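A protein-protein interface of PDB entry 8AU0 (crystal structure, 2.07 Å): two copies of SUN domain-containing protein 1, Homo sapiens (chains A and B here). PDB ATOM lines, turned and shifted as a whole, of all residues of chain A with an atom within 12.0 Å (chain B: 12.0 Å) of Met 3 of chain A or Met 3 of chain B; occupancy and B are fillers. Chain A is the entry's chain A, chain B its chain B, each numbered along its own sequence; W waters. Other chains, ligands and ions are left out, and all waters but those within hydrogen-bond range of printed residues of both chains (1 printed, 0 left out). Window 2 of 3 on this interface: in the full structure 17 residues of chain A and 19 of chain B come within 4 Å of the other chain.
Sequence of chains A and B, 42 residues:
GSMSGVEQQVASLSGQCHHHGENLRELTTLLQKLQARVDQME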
ATOM      1  N   SER A   2     -15.902  21.445  18.781  1.00  0.00           N
ATOM      2  CA  SER A   2     -16.619  20.427  19.542  1.00  0.00           C
ATOM      3  C   SER A   2     -15.870  20.071  20.824  1.00  0.00           C
ATOM      4  O   SER A   2     -14.732  19.600  20.771  1.00  0.00           O
ATOM      5  CB  SER A   2     -16.835  19.175  18.689  1.00  0.00           C
ATOM      6  OG  SER A   2     -17.415  18.128  19.449  1.00  0.00           O
ATOM      7  N   MET A   3     -16.515  20.309  21.972  1.00  0.00           N
ATOM      8  CA  MET A   3     -15.904  19.975  23.255  1.00  0.00           C
ATOM      9  C   MET A   3     -15.522  18.504  23.310  1.00  0.00           C
ATOM     10  O   MET A   3     -14.404  18.155  23.703  1.00  0.00           O
ATOM     11  CB  MET A   3     -16.857  20.316  24.402  1.00  0.00           C
ATOM     12  CG  MET A   3     -17.367  21.740  24.395  1.00  0.00           C
ATOM     13  SD  MET A   3     -16.061  22.964  24.586  1.00  0.00           S
ATOM     14  CE  MET A   3     -17.033  24.464  24.534  1.00  0.00           C
ATOM     15  N   SER A   4     -16.447  17.626  22.913  1.00  0.00           N
ATOM     16  CA  SER A   4     -16.165  16.196  22.903  1.00  0.00           C
ATOM     17  C   SER A   4     -14.991  15.877  21.989  1.00  0.00           C
ATOM     18  O   SER A   4     -14.130  15.061  22.335  1.00  0.00           O
ATOM     19  CB  SER A   4     -17.408  15.421  22.467  1.00  0.00           C
ATOM     20  OG  SER A   4     -18.548  15.830  23.197  1.00  0.00           O
ATOM     21  N   GLY A   5     -14.939  16.516  20.819  1.00  0.00           N
ATOM     22  CA  GLY A   5     -13.833  16.284  19.906  1.00  0.00           C
ATOM     23  C   GLY A   5     -12.488  16.632  20.516  1.00  0.00           C
ATOM     24  O   GLY A   5     -11.543  15.847  20.442  1.00  0.00           O
ATOM     25  N   VAL A   6     -12.395  17.811  21.134  1.00  0.00           N
ATOM     26  CA  VAL A   6     -11.146  18.219  21.773  1.00  0.00           C
ATOM     27  C   VAL A   6     -10.811  17.279  22.924  1.00  0.00           C
ATOM     28  O   VAL A   6      -9.644  16.936  23.139  1.00  0.00           O
ATOM     29  CB  VAL A   6     -11.240  19.685  22.237  1.00  0.00           C
ATOM     30  CG1 VAL A   6      -9.912  20.151  22.812  1.00  0.00           C
ATOM     31  CG2 VAL A   6     -11.663  20.577  21.086  1.00  0.00           C
ATOM     32  N   GLU A   7     -11.829  16.829  23.665  1.00  0.00           N
ATOM     33  CA  GLU A   7     -11.596  15.877  24.748  1.00  0.00           C
ATOM     34  C   GLU A   7     -10.984  14.583  24.225  1.00  0.00           C
ATOM     35  O   GLU A   7     -10.123  13.987  24.883  1.00  0.00           O
ATOM     36  CB  GLU A   7     -12.904  15.582  25.481  1.00  0.00           C
ATOM     37  CG  GLU A   7     -13.466  16.757  26.269  1.00  0.00           C
ATOM     38  CD  GLU A   7     -14.861  16.487  26.797  1.00  0.00           C
ATOM     39  OE1 GLU A   7     -15.569  15.656  26.189  1.00  0.00           O
ATOM     40  OE2 GLU A   7     -15.250  17.100  27.814  1.00  0.00           O
ATOM     41  N   GLN A   8     -11.413  14.135  23.042  1.00  0.00           N
ATOM     42  CA  GLN A   8     -10.871  12.901  22.482  1.00  0.00           C
ATOM     43  C   GLN A   8      -9.457  13.104  21.956  1.00  0.00           C
ATOM     44  O   GLN A   8      -8.624  12.192  22.030  1.00  0.00           O
ATOM     45  CB  GLN A   8     -11.788  12.381  21.377  1.00  0.00           C
ATOM     46  CG  GLN A   8     -13.172  12.006  21.867  1.00  0.00           C
ATOM     47  CD  GLN A   8     -14.267  12.474  20.931  1.00  0.00           C
ATOM     48  OE1 GLN A   8     -13.998  12.939  19.824  1.00  0.00           O
ATOM     49  NE2 GLN A   8     -15.513  12.358  21.376  1.00  0.00           N
ATOM     50  N   GLN A   9      -9.170  14.289  21.412  1.00  0.00           N
ATOM     51  CA  GLN A   9      -7.804  14.603  21.012  1.00  0.00           C
ATOM     52  C   GLN A   9      -6.866  14.612  22.213  1.00  0.00           C
ATOM     53  O   GLN A   9      -5.738  14.115  22.132  1.00  0.00           O
ATOM     54  CB  GLN A   9      -7.759  15.954  20.301  1.00  0.00           C
ATOM     55  CG  GLN A   9      -8.641  16.045  19.074  1.00  0.00           C
ATOM     56  CD  GLN A   9      -8.666  17.442  18.485  1.00  0.00           C
ATOM     57  OE1 GLN A   9      -7.658  18.149  18.491  1.00  0.00           O
ATOM     58  NE2 GLN A   9      -9.824  17.851  17.979  1.00  0.00           N
ATOM     59  N   VAL A  10      -7.315  15.179  23.335  1.00  0.00           N
ATOM     60  CA  VAL A  10      -6.461  15.255  24.516  1.00  0.00           C
ATOM     61  C   VAL A  10      -6.231  13.865  25.099  1.00  0.00           C
ATOM     62  O   VAL A  10      -5.148  13.565  25.613  1.00  0.00           O
ATOM     63  CB  VAL A  10      -7.063  16.222  25.552  1.00  0.00           C
ATOM     64  CG1 VAL A  10      -6.202  16.269  26.788  1.00  0.00           C
ATOM     65  CG2 VAL A  10      -7.185  17.614  24.967  1.00  0.00           C
ATOM     66  N   ALA A  11      -7.234  12.989  25.011  1.00  0.00           N
ATOM     67  CA  ALA A  11      -7.030  11.603  25.421  1.00  0.00           C
ATOM     68  C   ALA A  11      -6.048  10.895  24.495  1.00  0.00           C
ATOM     69  O   ALA A  11      -5.258  10.053  24.941  1.00  0.00           O
ATOM     70  CB  ALA A  11      -8.367  10.865  25.460  1.00  0.00           C
ATOM     71  N   SER A  12      -6.083  11.228  23.201  1.00  0.00           N
ATOM     72  CA  SER A  12      -5.116  10.678  22.256  1.00  0.00           C
ATOM     73  C   SER A  12      -3.700  11.093  22.629  1.00  0.00           C
ATOM     74  O   SER A  12      -2.804  10.249  22.760  1.00  0.00           O
ATOM     75  CB  SER A  12      -5.450  11.140  20.837  1.00  0.00           C
ATOM     76  OG  SER A  12      -4.535  10.604  19.899  1.00  0.00           O
ATOM     77  N   SER B   2     -12.731  30.447  22.972  1.00  0.00           N
ATOM     78  CA  SER B   2     -11.821  29.667  23.814  1.00  0.00           C
ATOM     79  C   SER B   2     -11.629  28.264  23.245  1.00  0.00           C
ATOM     80  O   SER B   2     -10.502  27.762  23.216  1.00  0.00           O
ATOM     81  CB  SER B   2     -12.333  29.583  25.259  1.00  0.00           C
ATOM     82  OG  SER B   2     -13.647  29.035  25.334  1.00  0.00           O
ATOM     83  N   MET B   3     -12.731  27.646  22.781  1.00  0.00           N
ATOM     84  CA  MET B   3     -12.646  26.296  22.226  1.00  0.00           C
ATOM     85  C   MET B   3     -11.631  26.228  21.097  1.00  0.00           C
ATOM     86  O   MET B   3     -10.939  25.220  20.938  1.00  0.00           O
ATOM     87  CB  MET B   3     -14.009  25.820  21.730  1.00  0.00           C
ATOM     88  CG  MET B   3     -13.925  24.566  20.881  1.00  0.00           C
ATOM     89  SD  MET B   3     -15.475  23.649  20.844  1.00  0.00           S
ATOM     90  CE  MET B   3     -16.674  24.954  21.090  1.00  0.00           C
ATOM     91  N   SER B   4     -11.511  27.293  20.313  1.00  0.00           N
ATOM     92  CA  SER B   4     -10.484  27.308  19.285  1.00  0.00           C
ATOM     93  C   SER B   4      -9.104  27.553  19.890  1.00  0.00           C
ATOM     94  O   SER B   4      -8.115  26.965  19.435  1.00  0.00           O
ATOM     95  CB  SER B   4     -10.829  28.362  18.241  1.00  0.00           C
ATOM     96  OG  SER B   4     -12.208  28.296  17.927  1.00  0.00           O
ATOM     97  N   GLY B   5      -9.018  28.407  20.918  1.00  0.00           N
ATOM     98  CA  GLY B   5      -7.756  28.576  21.628  1.00  0.00           C
ATOM     99  C   GLY B   5      -7.261  27.283  22.250  1.00  0.00           C
ATOM    100  O   GLY B   5      -6.056  27.002  22.263  1.00  0.00           O
ATOM    101  N   VAL B   6      -8.185  26.473  22.772  1.00  0.00           N
ATOM    102  CA  VAL B   6      -7.821  25.168  23.313  1.00  0.00           C
ATOM    103  C   VAL B   6      -7.425  24.215  22.192  1.00  0.00           C
ATOM    104  O   VAL B   6      -6.502  23.403  22.344  1.00  0.00           O
ATOM    105  CB  VAL B   6      -8.987  24.623  24.151  1.00  0.00           C
ATOM    106  CG1 VAL B   6      -8.801  23.165  24.455  1.00  0.00           C
ATOM    107  CG2 VAL B   6      -9.088  25.397  25.429  1.00  0.00           C
ATOM    108  N   GLU B   7      -8.103  24.296  21.046  1.00  0.00           N
ATOM    109  CA  GLU B   7      -7.724  23.450  19.919  1.00  0.00           C
ATOM    110  C   GLU B   7      -6.316  23.746  19.462  1.00  0.00           C
ATOM    111  O   GLU B   7      -5.651  22.869  18.899  1.00  0.00           O
ATOM    112  CB  GLU B   7      -8.686  23.629  18.750  1.00  0.00           C
ATOM    113  CG  GLU B   7      -9.792  22.574  18.722  1.00  0.00           C
ATOM    114  CD  GLU B   7     -10.955  22.962  17.834  1.00  0.00           C
ATOM    115  OE1 GLU B   7     -10.820  23.962  17.094  1.00  0.00           O
ATOM    116  OE2 GLU B   7     -12.002  22.273  17.884  1.00  0.00           O
ATOM    117  N   GLN B   8      -5.838  24.963  19.707  1.00  0.00           N
ATOM    118  CA  GLN B   8      -4.501  25.310  19.250  1.00  0.00           C
ATOM    119  C   GLN B   8      -3.445  24.786  20.195  1.00  0.00           C
ATOM    120  O   GLN B   8      -2.439  24.219  19.752  1.00  0.00           O
ATOM    121  CB  GLN B   8      -4.380  26.813  19.087  1.00  0.00           C
ATOM    122  CG  GLN B   8      -5.291  27.279  17.981  1.00  0.00           C
ATOM    123  CD  GLN B   8      -5.177  26.407  16.752  1.00  0.00           C
ATOM    124  OE1 GLN B   8      -4.103  26.291  16.149  1.00  0.00           O
ATOM    125  NE2 GLN B   8      -6.280  25.762  16.387  1.00  0.00           N
ATOM    126  N   GLN B   9      -3.639  24.995  21.496  1.00  0.00           N
ATOM    127  CA  GLN B   9      -2.721  24.432  22.479  1.00  0.00           C
ATOM    128  C   GLN B   9      -2.626  22.915  22.326  1.00  0.00           C
ATOM    129  O   GLN B   9      -1.521  22.350  22.324  1.00  0.00           O
ATOM    130  CB  GLN B   9      -3.167  24.857  23.882  1.00  0.00           C
ATOM    131  CG  GLN B   9      -3.292  26.385  23.996  1.00  0.00           C
ATOM    132  CD  GLN B   9      -4.024  26.862  25.234  1.00  0.00           C
ATOM    133  OE1 GLN B   9      -4.042  26.194  26.268  1.00  0.00           O
ATOM    134  NE2 GLN B   9      -4.637  28.027  25.129  1.00  0.00           N
ATOM    135  N   VAL B  10      -3.773  22.252  22.126  1.00  0.00           N
ATOM    136  CA  VAL B  10      -3.777  20.835  21.788  1.00  0.00           C
ATOM    137  C   VAL B  10      -2.933  20.584  20.546  1.00  0.00           C
ATOM    138  O   VAL B  10      -2.243  19.563  20.448  1.00  0.00           O
ATOM    139  CB  VAL B  10      -5.224  20.340  21.611  1.00  0.00           C
ATOM    140  CG1 VAL B  10      -5.240  18.950  21.025  1.00  0.00           C
ATOM    141  CG2 VAL B  10      -5.979  20.379  22.948  1.00  0.00           C
ATOM    142  N   ALA B  11      -2.944  21.527  19.591  1.00  0.00           N
ATOM    143  CA  ALA B  11      -2.162  21.360  18.361  1.00  0.00           C
ATOM    144  C   ALA B  11      -0.674  21.606  18.607  1.00  0.00           C
ATOM    145  O   ALA B  11       0.181  20.878  18.087  1.00  0.00           O
ATOM    146  CB  ALA B  11      -2.691  22.298  17.275  1.00  0.00           C
ATOM    147  N   SER B  12      -0.356  22.626  19.401  1.00  0.00           N
ATOM    148  CA  SER B  12       0.986  22.789  19.928  1.00  0.00           C
ATOM    149  C   SER B  12       1.510  21.478  20.506  1.00  0.00           C
ATOM    150  O   SER B  12       2.530  20.933  20.054  1.00  0.00           O
ATOM    151  CB  SER B  12       0.966  23.899  20.983  1.00  0.00           C
ATOM    152  OG  SER B  12       2.268  24.169  21.479  1.00  0.00           O
HETATM  153  O   HOH W   1     -12.652  19.784  17.703  1.00  0.00           O
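Met 3 of chain B touches its own counterpart, Met 3 of chain A.
Val 6 of chain B touches its own counterpart, Val 6 of chain A.
Val 6 of chain A touches Val 10 of chain B, but with the chains exchanged Val 10 of chain A does not touch Val 6 of chain B (5.8 Å).
Gln 9 of chain A touches Val 10 of chain B, but with the chains exchanged Val 10 of chain A does not touch Gln 9 of chain B (7.5 Å).
Water W1 bridges OE2 of Glu 7 of chain B (2.6 Å) and NE2 of Gln 9 of chain A (3.4 Å).
Hydrophobic or aromatic side chains of chain B within 4 Å of the printed part of chain A: Met 3, Val 6 and Val 10.
Of the 11 printed residues of chain A, 5 touch a printed residue of chain B.
Hydrophobic or aromatic side chains of chain A that line the printed part of chain B: Met 3, Val 6 and Val 10.
Among the printed residues, 7 pairs touch across the chains.
Among the printed residues, no Asp or Glu carboxylate lies within 4 Å of a Lys or Arg side-chain nitrogen of the other chain.
The side-chain sulfur (SD) of Met 3 of chain B lies within hydrogen-bond range of the backbone NH (N) of Ser 2 of chain A, at 3.0 Å.
The side-chain sulfur (SD) of Met 3 of chain B sits at hydrogen-bond distance from the backbone NH (N) of Met 3 of chain A, at 3.7 Å.
Val 6 of chain A touches Val 6 of chain B.
CG of Glu 7 of chain B touches CG2 of Val 6 of chain A, at 3.6 Å.
Val 10 of chain B touches Val 6 of chain A (CG2 to CG1, 3.9 Å).
CG1 of Val 10 of chain B touches OE1 of Gln 9 of chain A, 3.6 Å away.
CG2 of Val 10 of chain A touches CG2 of Val 10 of chain B, at 3.6 Å.
N of Gly 5 of chain A lies within hydrogen-bond range of OG of Ser 2 of chain A (3.3 Å).
Of chain B, only Met 3 comes within 4 Å of Met 3 of chain A.
No residue of chain B comes within 4 Å of Ser 4 of chain A.
Of the printed residues of chain B, Val 10 of chain A touches Val 10.
Printed residues of chain A within 4 Å of Met 3 of chain B: Ser 2 and Met 3.
No residue of chain A comes within 4 Å of Ser 4 of chain B.
No residue of chain A comes within 4 Å of Gly 5 of chain B.
Of chain A, only Val 6 (3.6 Å) comes within 4 Å of Val 6 of chain B.
Gln 9 of chain B touches none of the printed residues of chain A.
Of the printed residues of chain A, Val 10 of chain B touches Val 6, Gln 9 and Val 10.
The nearest residue of chain B that does not touch Met 3 of chain A is Ser 2 of chain B (5.7 Å).
The nearest residue of chain A that does not touch Met 3 of chain B is Val 6 of chain A (4.6 Å).
The nearest printed residue of chain B that does not touch Gln 9 of chain A is Glu 7 of chain B (4.8 Å).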
